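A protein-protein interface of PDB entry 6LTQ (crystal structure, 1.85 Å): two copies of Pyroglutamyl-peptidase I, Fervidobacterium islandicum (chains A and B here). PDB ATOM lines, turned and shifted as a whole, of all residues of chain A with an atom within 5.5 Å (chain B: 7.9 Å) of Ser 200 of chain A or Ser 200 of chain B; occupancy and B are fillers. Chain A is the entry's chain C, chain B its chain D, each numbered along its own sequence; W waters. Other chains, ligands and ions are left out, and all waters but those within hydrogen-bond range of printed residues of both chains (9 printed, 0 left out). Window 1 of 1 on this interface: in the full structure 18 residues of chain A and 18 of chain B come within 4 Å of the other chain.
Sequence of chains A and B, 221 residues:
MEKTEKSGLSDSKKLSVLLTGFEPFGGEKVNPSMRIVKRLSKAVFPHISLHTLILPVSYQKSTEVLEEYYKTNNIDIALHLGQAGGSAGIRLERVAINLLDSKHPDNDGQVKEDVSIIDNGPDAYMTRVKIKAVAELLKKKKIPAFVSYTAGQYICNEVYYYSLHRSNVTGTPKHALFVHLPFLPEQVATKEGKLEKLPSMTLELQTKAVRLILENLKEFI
Hydrophobic or aromatic side chains of chain B within 4 Å of the printed part of chain A: Ala 88, Pro 144, Pro 185, Val 188, Pro 199 and Leu 205.
Along chain A the printed residues that touch a printed residue of chain B span positions 88 to 202.
Among the printed residues, 17 pairs touch across the chains.
Leu 198 of chain B touches Ala 88 of chain A (O to CB, 3.4 Å).
Pro 144 of chain A touches Pro 185 of chain B.
CB of Pro 144 of chain A touches CG1 of Val 188 of chain B, at 3.8 Å.
Pro 144 of chain A touches Ser 200 of chain B (CG to OG, 3.98 Å).
Leu 205 of chain B touches Pro 185 of chain A (CD2 to CG, 3.7 Å).
Val 188 of chain A touches Pro 144 of chain B (CG1 to CB, 3.9 Å).
CB of Ala 88 of chain B touches O of Leu 198 of chain A (3.5 Å).
Pro 199 of chain B touches Pro 199 of chain A (CB to CB, 3.9 Å).
Ser 200 of chain A touches Pro 144 of chain B.
CG2 of Thr 202 of chain B touches OG1 of Thr 202 of chain A, 3.5 Å away.
The side-chain hydroxyl (OG1) of Thr 202 of chain B is in hydrogen-bond range of the backbone NH (N) of Leu 205 of chain B (3.2 Å).
Water W6 lies within hydrogen-bond range of OG of Ser 200 of chain A (2.6 Å), O of Leu 198 of chain A (2.8 Å) and O of Ala 88 of chain B (2.8 Å).
Water W1 lies within hydrogen-bond range of the backbone carbonyl oxygen (O) of Ala 88 of chain A (2.8 Å), the backbone carbonyl oxygen (O) of Leu 198 of chain B (2.8 Å) and the side-chain hydroxyl (OG) of Ser 200 of chain B (2.8 Å).
Water W4 bridges OG1 of Thr 202 of chain A and OG1 of Thr 202 of chain B.
Water W3 lies within hydrogen-bond range of O of Ser 200 of chain A (2.8 Å), O of Ala 88 of chain A (2.9 Å) and N of Ser 200 of chain B (3.0 Å).
Water W2 lies within hydrogen-bond range of the side-chain hydroxyl (OG) of Ser 200 of chain B (2.9 Å) and the backbone carbonyl oxygen (O) of Ser 200 of chain A (3.0 Å).
Water W8 bridges the side-chain hydroxyl (OG) of Ser 200 of chain A and the backbone carbonyl oxygen (O) of Ser 200 of chain B.
Of chain B, only Pro 144 (3.9 Å) and Ser 200 (3.4 Å) come within 4 Å of Ser 200 of chain A.
Ser 200 of chain B touches two residues of chain A.
Printed residues of chain A within 4 Å of Lys 142 of chain B: Pro 185.
Of the printed residues of chain B, Pro 185 of chain A touches Lys 142, Pro 144 and Leu 205.
Of the printed residues of chain A, Pro 199 of chain B touches Ala 88 and Pro 199.
Of the printed residues of chain B, Ala 88 of chain A touches Lys 197 (3.3 Å), Leu 198 (3.4 Å) and Pro 199 (3.7 Å).
The backbone carbonyl oxygen of Ser 200 of chain B sits close to the backbone carbonyl oxygen of Ser 200 of chain A (3.4 Å).
Pro 144 of chain A touches Pro 185 of chain B, and with the chains exchanged Pro 185 of chain A touches Pro 144 of chain B.
Pro 144 of chain A touches Ser 200 of chain B, and with the chains exchanged Ser 200 of chain A touches Pro 144 of chain B.
Pro 199 of chain B touches its own counterpart, Pro 199 of chain A.
Thr 202 of chain A touches its own counterpart, Thr 202 of chain B.
Positions printed for both chains: 87, 88, 144, 182, 183, 184, 185, 188, 198, 199, 200, 201, 202 and 206.
Of the 17 pairs that touch across the chains among the printed residues, 13 have their exchanged pair printed and touching as well.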
ATOM      1  N   SER A  87     -12.250 -27.049 -17.097  1.00  0.00           N
ATOM      2  CA  SER A  87     -12.982 -28.288 -17.309  1.00  0.00           C
ATOM      3  C   SER A  87     -13.287 -28.461 -18.791  1.00  0.00           C
ATOM      4  O   SER A  87     -13.453 -27.492 -19.524  1.00  0.00           O
ATOM      5  CB  SER A  87     -14.286 -28.292 -16.495  1.00  0.00           C
ATOM      6  OG  SER A  87     -13.964 -28.407 -15.104  1.00  0.00           O
ATOM      7  N   ALA A  88     -13.302 -29.712 -19.236  1.00  0.00           N
ATOM      8  CA  ALA A  88     -13.425 -30.003 -20.663  1.00  0.00           C
ATOM      9  C   ALA A  88     -14.808 -30.465 -21.074  1.00  0.00           C
ATOM     10  O   ALA A  88     -15.084 -30.540 -22.282  1.00  0.00           O
ATOM     11  CB  ALA A  88     -12.407 -31.076 -21.076  1.00  0.00           C
ATOM     12  N   PRO A 144     -19.842 -34.538 -24.242  1.00  0.00           N
ATOM     13  CA  PRO A 144     -18.988 -34.935 -23.112  1.00  0.00           C
ATOM     14  C   PRO A 144     -19.559 -34.424 -21.796  1.00  0.00           C
ATOM     15  O   PRO A 144     -19.911 -33.253 -21.656  1.00  0.00           O
ATOM     16  CB  PRO A 144     -17.636 -34.283 -23.441  1.00  0.00           C
ATOM     17  CG  PRO A 144     -17.665 -34.112 -24.924  1.00  0.00           C
ATOM     18  CD  PRO A 144     -19.104 -33.798 -25.276  1.00  0.00           C
ATOM     19  N   PRO A 182     -17.378 -25.618 -19.067  1.00  0.00           N
ATOM     20  CA  PRO A 182     -16.089 -25.196 -19.625  1.00  0.00           C
ATOM     21  C   PRO A 182     -16.103 -23.721 -19.983  1.00  0.00           C
ATOM     22  O   PRO A 182     -17.157 -23.111 -20.184  1.00  0.00           O
ATOM     23  CB  PRO A 182     -15.947 -26.051 -20.898  1.00  0.00           C
ATOM     24  CG  PRO A 182     -16.911 -27.236 -20.672  1.00  0.00           C
ATOM     25  CD  PRO A 182     -18.053 -26.623 -19.910  1.00  0.00           C
ATOM     26  N   PHE A 183     -14.890 -23.163 -20.073  1.00  0.00           N
ATOM     27  CA  PHE A 183     -14.679 -21.894 -20.758  1.00  0.00           C
ATOM     28  C   PHE A 183     -15.319 -21.936 -22.145  1.00  0.00           C
ATOM     29  O   PHE A 183     -15.357 -22.984 -22.808  1.00  0.00           O
ATOM     30  CB  PHE A 183     -13.177 -21.636 -20.922  1.00  0.00           C
ATOM     31  CG  PHE A 183     -12.498 -21.020 -19.727  1.00  0.00           C
ATOM     32  CD1 PHE A 183     -13.103 -19.998 -18.998  1.00  0.00           C
ATOM     33  CD2 PHE A 183     -11.201 -21.409 -19.398  1.00  0.00           C
ATOM     34  CE1 PHE A 183     -12.440 -19.387 -17.935  1.00  0.00           C
ATOM     35  CE2 PHE A 183     -10.531 -20.803 -18.341  1.00  0.00           C
ATOM     36  CZ  PHE A 183     -11.158 -19.787 -17.607  1.00  0.00           C
ATOM     37  N   LEU A 184     -15.847 -20.789 -22.572  1.00  0.00           N
ATOM     38  CA  LEU A 184     -16.155 -20.575 -23.975  1.00  0.00           C
ATOM     39  C   LEU A 184     -14.855 -20.446 -24.762  1.00  0.00           C
ATOM     40  O   LEU A 184     -13.848 -19.967 -24.232  1.00  0.00           O
ATOM     41  CB  LEU A 184     -16.983 -19.300 -24.162  1.00  0.00           C
ATOM     42  CG  LEU A 184     -18.343 -19.217 -23.466  1.00  0.00           C
ATOM     43  CD1 LEU A 184     -19.004 -17.909 -23.783  1.00  0.00           C
ATOM     44  CD2 LEU A 184     -19.226 -20.410 -23.887  1.00  0.00           C
ATOM     45  N   PRO A 185     -14.845 -20.834 -26.037  1.00  0.00           N
ATOM     46  CA  PRO A 185     -13.604 -20.692 -26.822  1.00  0.00           C
ATOM     47  C   PRO A 185     -13.032 -19.284 -26.823  1.00  0.00           C
ATOM     48  O   PRO A 185     -11.809 -19.123 -26.763  1.00  0.00           O
ATOM     49  CB  PRO A 185     -14.024 -21.139 -28.226  1.00  0.00           C
ATOM     50  CG  PRO A 185     -15.114 -22.155 -27.965  1.00  0.00           C
ATOM     51  CD  PRO A 185     -15.874 -21.606 -26.762  1.00  0.00           C
ATOM     52  N   VAL A 188     -10.673 -18.727 -23.891  1.00  0.00           N
ATOM     53  CA  VAL A 188      -9.342 -19.317 -23.977  1.00  0.00           C
ATOM     54  C   VAL A 188      -8.511 -18.611 -25.035  1.00  0.00           C
ATOM     55  O   VAL A 188      -7.287 -18.486 -24.891  1.00  0.00           O
ATOM     56  CB  VAL A 188      -9.446 -20.826 -24.266  1.00  0.00           C
ATOM     57  CG1 VAL A 188      -8.061 -21.429 -24.531  1.00  0.00           C
ATOM     58  CG2 VAL A 188     -10.128 -21.521 -23.090  1.00  0.00           C
ATOM     59  N   LEU A 198      -5.902 -24.411 -22.745  1.00  0.00           N
ATOM     60  CA  LEU A 198      -7.006 -24.884 -21.921  1.00  0.00           C
ATOM     61  C   LEU A 198      -8.164 -25.393 -22.774  1.00  0.00           C
ATOM     62  O   LEU A 198      -8.372 -24.920 -23.897  1.00  0.00           O
ATOM     63  CB  LEU A 198      -7.527 -23.770 -21.042  1.00  0.00           C
ATOM     64  CG  LEU A 198      -6.617 -23.428 -19.862  1.00  0.00           C
ATOM     65  CD1 LEU A 198      -7.128 -22.169 -19.234  1.00  0.00           C
ATOM     66  CD2 LEU A 198      -6.607 -24.568 -18.865  1.00  0.00           C
ATOM     67  N   PRO A 199      -8.965 -26.308 -22.230  1.00  0.00           N
ATOM     68  CA  PRO A 199     -10.160 -26.799 -22.932  1.00  0.00           C
ATOM     69  C   PRO A 199     -11.265 -25.752 -22.978  1.00  0.00           C
ATOM     70  O   PRO A 199     -11.314 -24.815 -22.181  1.00  0.00           O
ATOM     71  CB  PRO A 199     -10.623 -27.995 -22.079  1.00  0.00           C
ATOM     72  CG  PRO A 199      -9.569 -28.213 -21.044  1.00  0.00           C
ATOM     73  CD  PRO A 199      -8.785 -26.944 -20.913  1.00  0.00           C
ATOM     74  N   SER A 200     -12.172 -25.938 -23.930  1.00  0.00           N
ATOM     75  CA  SER A 200     -13.332 -25.070 -24.068  1.00  0.00           C
ATOM     76  C   SER A 200     -14.466 -25.855 -24.715  1.00  0.00           C
ATOM     77  O   SER A 200     -14.284 -26.977 -25.198  1.00  0.00           O
ATOM     78  CB  SER A 200     -13.010 -23.833 -24.918  1.00  0.00           C
ATOM     79  OG  SER A 200     -12.554 -24.271 -26.203  1.00  0.00           O
ATOM     80  N   MET A 201     -15.642 -25.234 -24.740  1.00  0.00           N
ATOM     81  CA  MET A 201     -16.802 -25.788 -25.435  1.00  0.00           C
ATOM     82  C   MET A 201     -17.637 -24.621 -25.949  1.00  0.00           C
ATOM     83  O   MET A 201     -17.902 -23.664 -25.207  1.00  0.00           O
ATOM     84  CB  MET A 201     -17.632 -26.695 -24.505  1.00  0.00           C
ATOM     85  CG  MET A 201     -18.809 -27.421 -25.188  1.00  0.00           C
ATOM     86  SD  MET A 201     -19.652 -28.498 -24.020  1.00  0.00           S
ATOM     87  CE  MET A 201     -18.523 -29.915 -23.948  1.00  0.00           C
ATOM     88  N   THR A 202     -18.030 -24.688 -27.220  1.00  0.00           N
ATOM     89  CA  THR A 202     -18.775 -23.585 -27.824  1.00  0.00           C
ATOM     90  C   THR A 202     -20.073 -23.321 -27.066  1.00  0.00           C
ATOM     91  O   THR A 202     -20.670 -24.220 -26.463  1.00  0.00           O
ATOM     92  CB  THR A 202     -19.114 -23.884 -29.284  1.00  0.00           C
ATOM     93  OG1 THR A 202     -19.988 -25.021 -29.341  1.00  0.00           O
ATOM     94  CG2 THR A 202     -17.854 -24.155 -30.097  1.00  0.00           C
ATOM     95  N   GLN A 206     -22.795 -25.980 -25.293  1.00  0.00           N
ATOM     96  CA  GLN A 206     -23.166 -25.870 -23.886  1.00  0.00           C
ATOM     97  C   GLN A 206     -24.656 -25.585 -23.731  1.00  0.00           C
ATOM     98  O   GLN A 206     -25.312 -26.145 -22.843  1.00  0.00           O
ATOM     99  CB  GLN A 206     -22.347 -24.778 -23.197  1.00  0.00           C
ATOM    100  CG  GLN A 206     -20.840 -25.028 -23.162  1.00  0.00           C
ATOM    101  CD  GLN A 206     -20.169 -24.116 -22.164  1.00  0.00           C
ATOM    102  OE1 GLN A 206     -20.814 -23.689 -21.207  1.00  0.00           O
ATOM    103  NE2 GLN A 206     -18.876 -23.797 -22.377  1.00  0.00           N
ATOM    104  N   GLY B  86      -6.828 -35.433 -27.325  1.00  0.00           N
ATOM    105  CA  GLY B  86      -6.292 -34.869 -26.108  1.00  0.00           C
ATOM    106  C   GLY B  86      -5.890 -33.411 -26.222  1.00  0.00           C
ATOM    107  O   GLY B  86      -5.724 -32.747 -25.187  1.00  0.00           O
ATOM    108  N   SER B  87      -5.691 -32.902 -27.435  1.00  0.00           N
ATOM    109  CA  SER B  87      -5.388 -31.484 -27.601  1.00  0.00           C
ATOM    110  C   SER B  87      -6.659 -30.643 -27.492  1.00  0.00           C
ATOM    111  O   SER B  87      -7.741 -31.053 -27.920  1.00  0.00           O
ATOM    112  CB  SER B  87      -4.686 -31.240 -28.936  1.00  0.00           C
ATOM    113  OG  SER B  87      -3.375 -31.794 -28.887  1.00  0.00           O
ATOM    114  N   ALA B  88      -6.519 -29.444 -26.939  1.00  0.00           N
ATOM    115  CA  ALA B  88      -7.682 -28.637 -26.597  1.00  0.00           C
ATOM    116  C   ALA B  88      -7.964 -27.534 -27.602  1.00  0.00           C
ATOM    117  O   ALA B  88      -9.053 -26.951 -27.561  1.00  0.00           O
ATOM    118  CB  ALA B  88      -7.496 -27.991 -25.218  1.00  0.00           C
ATOM    119  N   GLY B  89      -7.007 -27.217 -28.472  1.00  0.00           N
ATOM    120  CA  GLY B  89      -7.170 -26.125 -29.419  1.00  0.00           C
ATOM    121  C   GLY B  89      -6.594 -26.477 -30.782  1.00  0.00           C
ATOM    122  O   GLY B  89      -6.097 -27.577 -30.999  1.00  0.00           O
ATOM    123  N   LYS B 142     -11.180 -15.404 -32.097  1.00  0.00           N
ATOM    124  CA  LYS B 142     -11.762 -16.049 -30.911  1.00  0.00           C
ATOM    125  C   LYS B 142     -11.712 -17.574 -30.969  1.00  0.00           C
ATOM    126  O   LYS B 142     -12.568 -18.257 -30.389  1.00  0.00           O
ATOM    127  CB  LYS B 142     -13.201 -15.581 -30.663  1.00  0.00           C
ATOM    128  CG  LYS B 142     -13.337 -14.051 -30.582  1.00  0.00           C
ATOM    129  CD  LYS B 142     -14.775 -13.664 -30.287  1.00  0.00           C
ATOM    130  CE  LYS B 142     -14.990 -12.176 -30.491  1.00  0.00           C
ATOM    131  NZ  LYS B 142     -14.115 -11.372 -29.601  1.00  0.00           N
ATOM    132  N   ILE B 143     -10.719 -18.129 -31.650  1.00  0.00           N
ATOM    133  CA  ILE B 143     -10.558 -19.574 -31.739  1.00  0.00           C
ATOM    134  C   ILE B 143      -9.291 -19.964 -30.991  1.00  0.00           C
ATOM    135  O   ILE B 143      -8.196 -19.501 -31.353  1.00  0.00           O
ATOM    136  CB  ILE B 143     -10.515 -20.050 -33.200  1.00  0.00           C
ATOM    137  CG1 ILE B 143     -11.792 -19.609 -33.933  1.00  0.00           C
ATOM    138  CG2 ILE B 143     -10.377 -21.551 -33.255  1.00  0.00           C
ATOM    139  CD1 ILE B 143     -11.878 -20.093 -35.396  1.00  0.00           C
ATOM    140  N   PRO B 144      -9.362 -20.835 -29.986  1.00  0.00           N
ATOM    141  CA  PRO B 144      -8.141 -21.297 -29.308  1.00  0.00           C
ATOM    142  C   PRO B 144      -7.175 -21.951 -30.291  1.00  0.00           C
ATOM    143  O   PRO B 144      -7.561 -22.809 -31.085  1.00  0.00           O
ATOM    144  CB  PRO B 144      -8.662 -22.310 -28.274  1.00  0.00           C
ATOM    145  CG  PRO B 144     -10.080 -21.898 -28.038  1.00  0.00           C
ATOM    146  CD  PRO B 144     -10.591 -21.356 -29.359  1.00  0.00           C
ATOM    147  N   LEU B 181      -5.760 -31.384 -34.719  1.00  0.00           N
ATOM    148  CA  LEU B 181      -7.125 -31.049 -34.359  1.00  0.00           C
ATOM    149  C   LEU B 181      -7.568 -31.799 -33.105  1.00  0.00           C
ATOM    150  O   LEU B 181      -7.228 -32.983 -32.924  1.00  0.00           O
ATOM    151  CB  LEU B 181      -8.099 -31.404 -35.505  1.00  0.00           C
ATOM    152  CG  LEU B 181      -7.777 -30.775 -36.852  1.00  0.00           C
ATOM    153  CD1 LEU B 181      -8.564 -31.535 -37.957  1.00  0.00           C
ATOM    154  CD2 LEU B 181      -8.118 -29.288 -36.832  1.00  0.00           C
ATOM    155  N   PRO B 182      -8.356 -31.139 -32.254  1.00  0.00           N
ATOM    156  CA  PRO B 182      -8.943 -31.829 -31.098  1.00  0.00           C
ATOM    157  C   PRO B 182      -9.870 -32.954 -31.531  1.00  0.00           C
ATOM    158  O   PRO B 182     -10.354 -32.991 -32.660  1.00  0.00           O
ATOM    159  CB  PRO B 182      -9.748 -30.722 -30.384  1.00  0.00           C
ATOM    160  CG  PRO B 182      -9.100 -29.415 -30.816  1.00  0.00           C
ATOM    161  CD  PRO B 182      -8.642 -29.688 -32.258  1.00  0.00           C
ATOM    162  N   PHE B 183     -10.123 -33.872 -30.599  1.00  0.00           N
ATOM    163  CA  PHE B 183     -11.275 -34.762 -30.730  1.00  0.00           C
ATOM    164  C   PHE B 183     -12.544 -33.955 -30.990  1.00  0.00           C
ATOM    165  O   PHE B 183     -12.713 -32.842 -30.478  1.00  0.00           O
ATOM    166  CB  PHE B 183     -11.481 -35.553 -29.446  1.00  0.00           C
ATOM    167  CG  PHE B 183     -10.687 -36.812 -29.351  1.00  0.00           C
ATOM    168  CD1 PHE B 183     -10.539 -37.655 -30.444  1.00  0.00           C
ATOM    169  CD2 PHE B 183     -10.139 -37.181 -28.148  1.00  0.00           C
ATOM    170  CE1 PHE B 183      -9.845 -38.843 -30.325  1.00  0.00           C
ATOM    171  CE2 PHE B 183      -9.426 -38.375 -28.024  1.00  0.00           C
ATOM    172  CZ  PHE B 183      -9.286 -39.200 -29.116  1.00  0.00           C
ATOM    173  N   LEU B 184     -13.452 -34.525 -31.785  1.00  0.00           N
ATOM    174  CA  LEU B 184     -14.819 -34.036 -31.803  1.00  0.00           C
ATOM    175  C   LEU B 184     -15.513 -34.409 -30.493  1.00  0.00           C
ATOM    176  O   LEU B 184     -15.176 -35.421 -29.870  1.00  0.00           O
ATOM    177  CB  LEU B 184     -15.610 -34.632 -32.980  1.00  0.00           C
ATOM    178  CG  LEU B 184     -15.097 -34.287 -34.384  1.00  0.00           C
ATOM    179  CD1 LEU B 184     -15.853 -35.122 -35.432  1.00  0.00           C
ATOM    180  CD2 LEU B 184     -15.222 -32.800 -34.705  1.00  0.00           C
ATOM    181  N   PRO B 185     -16.495 -33.618 -30.063  1.00  0.00           N
ATOM    182  CA  PRO B 185     -17.218 -33.972 -28.828  1.00  0.00           C
ATOM    183  C   PRO B 185     -17.793 -35.384 -28.860  1.00  0.00           C
ATOM    184  O   PRO B 185     -17.732 -36.097 -27.845  1.00  0.00           O
ATOM    185  CB  PRO B 185     -18.308 -32.901 -28.744  1.00  0.00           C
ATOM    186  CG  PRO B 185     -17.747 -31.736 -29.514  1.00  0.00           C
ATOM    187  CD  PRO B 185     -16.950 -32.348 -30.646  1.00  0.00           C
ATOM    188  N   GLU B 186     -18.281 -35.846 -30.016  1.00  0.00           N
ATOM    189  CA  GLU B 186     -18.829 -37.205 -30.063  1.00  0.00           C
ATOM    190  C   GLU B 186     -17.774 -38.271 -29.772  1.00  0.00           C
ATOM    191  O   GLU B 186     -18.106 -39.349 -29.258  1.00  0.00           O
ATOM    192  CB  GLU B 186     -19.477 -37.456 -31.420  1.00  0.00           C
ATOM    193  CG  GLU B 186     -18.497 -37.410 -32.560  1.00  0.00           C
ATOM    194  CD  GLU B 186     -19.185 -37.213 -33.885  1.00  0.00           C
ATOM    195  OE1 GLU B 186     -19.401 -38.226 -34.591  1.00  0.00           O
ATOM    196  OE2 GLU B 186     -19.515 -36.050 -34.211  1.00  0.00           O
ATOM    197  N   GLN B 187     -16.498 -37.992 -30.072  1.00  0.00           N
ATOM    198  CA  GLN B 187     -15.436 -38.953 -29.776  1.00  0.00           C
ATOM    199  C   GLN B 187     -15.113 -39.007 -28.289  1.00  0.00           C
ATOM    200  O   GLN B 187     -14.636 -40.036 -27.799  1.00  0.00           O
ATOM    201  CB  GLN B 187     -14.153 -38.614 -30.547  1.00  0.00           C
ATOM    202  CG  GLN B 187     -14.324 -38.651 -32.071  1.00  0.00           C
ATOM    203  CD  GLN B 187     -13.068 -38.243 -32.821  1.00  0.00           C
ATOM    204  OE1 GLN B 187     -12.811 -37.054 -33.013  1.00  0.00           O
ATOM    205  NE2 GLN B 187     -12.276 -39.239 -33.255  1.00  0.00           N
ATOM    206  N   VAL B 188     -15.306 -37.901 -27.568  1.00  0.00           N
ATOM    207  CA  VAL B 188     -15.065 -37.944 -26.126  1.00  0.00           C
ATOM    208  C   VAL B 188     -16.278 -38.510 -25.414  1.00  0.00           C
ATOM    209  O   VAL B 188     -16.145 -39.178 -24.381  1.00  0.00           O
ATOM    210  CB  VAL B 188     -14.693 -36.550 -25.592  1.00  0.00           C
ATOM    211  CG1 VAL B 188     -14.608 -36.532 -24.041  1.00  0.00           C
ATOM    212  CG2 VAL B 188     -13.354 -36.094 -26.203  1.00  0.00           C
ATOM    213  N   ALA B 189     -17.469 -38.277 -25.960  1.00  0.00           N
ATOM    214  CA  ALA B 189     -18.687 -38.730 -25.292  1.00  0.00           C
ATOM    215  C   ALA B 189     -18.734 -40.251 -25.111  1.00  0.00           C
ATOM    216  O   ALA B 189     -19.433 -40.730 -24.211  1.00  0.00           O
ATOM    217  CB  ALA B 189     -19.898 -38.225 -26.068  1.00  0.00           C
ATOM    218  N   LYS B 197     -13.135 -37.112 -19.624  1.00  0.00           N
ATOM    219  CA  LYS B 197     -12.795 -35.729 -19.317  1.00  0.00           C
ATOM    220  C   LYS B 197     -11.850 -35.101 -20.336  1.00  0.00           C
ATOM    221  O   LYS B 197     -11.324 -34.018 -20.084  1.00  0.00           O
ATOM    222  CB  LYS B 197     -12.169 -35.639 -17.924  1.00  0.00           C
ATOM    223  CG  LYS B 197     -13.054 -36.181 -16.823  1.00  0.00           C
ATOM    224  CD  LYS B 197     -12.391 -36.039 -15.467  1.00  0.00           C
ATOM    225  CE  LYS B 197     -13.422 -36.065 -14.350  1.00  0.00           C
ATOM    226  NZ  LYS B 197     -12.789 -35.854 -13.014  1.00  0.00           N
ATOM    227  N   LEU B 198     -11.629 -35.745 -21.479  1.00  0.00           N
ATOM    228  CA  LEU B 198     -10.724 -35.192 -22.479  1.00  0.00           C
ATOM    229  C   LEU B 198     -11.304 -33.934 -23.127  1.00  0.00           C
ATOM    230  O   LEU B 198     -12.526 -33.761 -23.193  1.00  0.00           O
ATOM    231  CB  LEU B 198     -10.433 -36.232 -23.551  1.00  0.00           C
ATOM    232  CG  LEU B 198      -9.490 -37.354 -23.099  1.00  0.00           C
ATOM    233  CD1 LEU B 198      -9.418 -38.446 -24.158  1.00  0.00           C
ATOM    234  CD2 LEU B 198      -8.099 -36.825 -22.724  1.00  0.00           C
ATOM    235  N   PRO B 199     -10.448 -33.041 -23.633  1.00  0.00           N
ATOM    236  CA  PRO B 199     -10.932 -31.860 -24.360  1.00  0.00           C
ATOM    237  C   PRO B 199     -11.472 -32.214 -25.740  1.00  0.00           C
ATOM    238  O   PRO B 199     -11.099 -33.218 -26.340  1.00  0.00           O
ATOM    239  CB  PRO B 199      -9.687 -30.963 -24.494  1.00  0.00           C
ATOM    240  CG  PRO B 199      -8.622 -31.565 -23.635  1.00  0.00           C
ATOM    241  CD  PRO B 199      -8.981 -33.033 -23.451  1.00  0.00           C
ATOM    242  N   SER B 200     -12.318 -31.325 -26.267  1.00  0.00           N
ATOM    243  CA  SER B 200     -12.883 -31.513 -27.599  1.00  0.00           C
ATOM    244  C   SER B 200     -13.167 -30.152 -28.218  1.00  0.00           C
ATOM    245  O   SER B 200     -13.082 -29.120 -27.557  1.00  0.00           O
ATOM    246  CB  SER B 200     -14.152 -32.373 -27.526  1.00  0.00           C
ATOM    247  OG  SER B 200     -15.163 -31.672 -26.821  1.00  0.00           O
ATOM    248  N   MET B 201     -13.504 -30.151 -29.511  1.00  0.00           N
ATOM    249  CA  MET B 201     -13.927 -28.924 -30.174  1.00  0.00           C
ATOM    250  C   MET B 201     -14.931 -29.309 -31.253  1.00  0.00           C
ATOM    251  O   MET B 201     -14.695 -30.272 -31.987  1.00  0.00           O
ATOM    252  CB  MET B 201     -12.730 -28.164 -30.773  1.00  0.00           C
ATOM    253  CG  MET B 201     -13.084 -26.797 -31.412  1.00  0.00           C
ATOM    254  SD  MET B 201     -11.614 -26.018 -32.127  1.00  0.00           S
ATOM    255  CE  MET B 201     -10.841 -25.302 -30.662  1.00  0.00           C
ATOM    256  N   THR B 202     -16.058 -28.599 -31.312  1.00  0.00           N
ATOM    257  CA  THR B 202     -17.102 -28.980 -32.266  1.00  0.00           C
ATOM    258  C   THR B 202     -16.576 -28.959 -33.696  1.00  0.00           C
ATOM    259  O   THR B 202     -15.650 -28.214 -34.035  1.00  0.00           O
ATOM    260  CB  THR B 202     -18.325 -28.053 -32.168  1.00  0.00           C
ATOM    261  OG1 THR B 202     -17.971 -26.727 -32.580  1.00  0.00           O
ATOM    262  CG2 THR B 202     -18.882 -28.018 -30.744  1.00  0.00           C
ATOM    263  N   LEU B 203     -17.196 -29.793 -34.542  1.00  0.00           N
ATOM    264  CA  LEU B 203     -16.855 -29.794 -35.964  1.00  0.00           C
ATOM    265  C   LEU B 203     -17.047 -28.412 -36.565  1.00  0.00           C
ATOM    266  O   LEU B 203     -16.233 -27.955 -37.388  1.00  0.00           O
ATOM    267  CB  LEU B 203     -17.719 -30.819 -36.710  1.00  0.00           C
ATOM    268  CG  LEU B 203     -17.455 -30.901 -38.222  1.00  0.00           C
ATOM    269  CD1 LEU B 203     -16.029 -31.419 -38.520  1.00  0.00           C
ATOM    270  CD2 LEU B 203     -18.508 -31.788 -38.878  1.00  0.00           C
ATOM    271  N   LEU B 205     -16.682 -25.416 -35.212  1.00  0.00           N
ATOM    272  CA  LEU B 205     -15.584 -24.502 -34.895  1.00  0.00           C
ATOM    273  C   LEU B 205     -14.279 -24.944 -35.555  1.00  0.00           C
ATOM    274  O   LEU B 205     -13.524 -24.104 -36.067  1.00  0.00           O
ATOM    275  CB  LEU B 205     -15.418 -24.380 -33.373  1.00  0.00           C
ATOM    276  CG  LEU B 205     -14.424 -23.305 -32.911  1.00  0.00           C
ATOM    277  CD1 LEU B 205     -14.796 -21.907 -33.436  1.00  0.00           C
ATOM    278  CD2 LEU B 205     -14.286 -23.307 -31.372  1.00  0.00           C
ATOM    279  N   GLN B 206     -13.999 -26.252 -35.577  1.00  0.00           N
ATOM    280  CA  GLN B 206     -12.797 -26.727 -36.269  1.00  0.00           C
ATOM    281  C   GLN B 206     -12.854 -26.389 -37.758  1.00  0.00           C
ATOM    282  O   GLN B 206     -11.848 -25.994 -38.359  1.00  0.00           O
ATOM    283  CB  GLN B 206     -12.628 -28.237 -36.103  1.00  0.00           C
ATOM    284  CG  GLN B 206     -12.445 -28.717 -34.683  1.00  0.00           C
ATOM    285  CD  GLN B 206     -11.882 -30.105 -34.649  1.00  0.00           C
ATOM    286  OE1 GLN B 206     -11.136 -30.506 -35.550  1.00  0.00           O
ATOM    287  NE2 GLN B 206     -12.232 -30.860 -33.620  1.00  0.00           N
HETATM  288  O   HOH W   1     -14.815 -32.544 -24.151  1.00  0.00           O
HETATM  289  O   HOH W   2     -15.988 -28.944 -26.611  1.00  0.00           O
HETATM  290  O   HOH W   3     -13.256 -29.426 -24.208  1.00  0.00           O
HETATM  291  O   HOH W   4     -20.328 -25.255 -32.124  1.00  0.00           O
HETATM  292  O   HOH W   5     -11.091 -27.854 -25.931  1.00  0.00           O
HETATM  293  O   HOH W   6      -9.949 -24.618 -26.214  1.00  0.00           O
HETATM  294  O   HOH W   7     -16.368 -26.927 -28.695  1.00  0.00           O
HETATM  295  O   HOH W   8     -13.678 -26.204 -28.012  1.00  0.00           O
HETATM  296  O   HOH W   9      -6.615 -24.670 -26.327  1.00  0.00           O
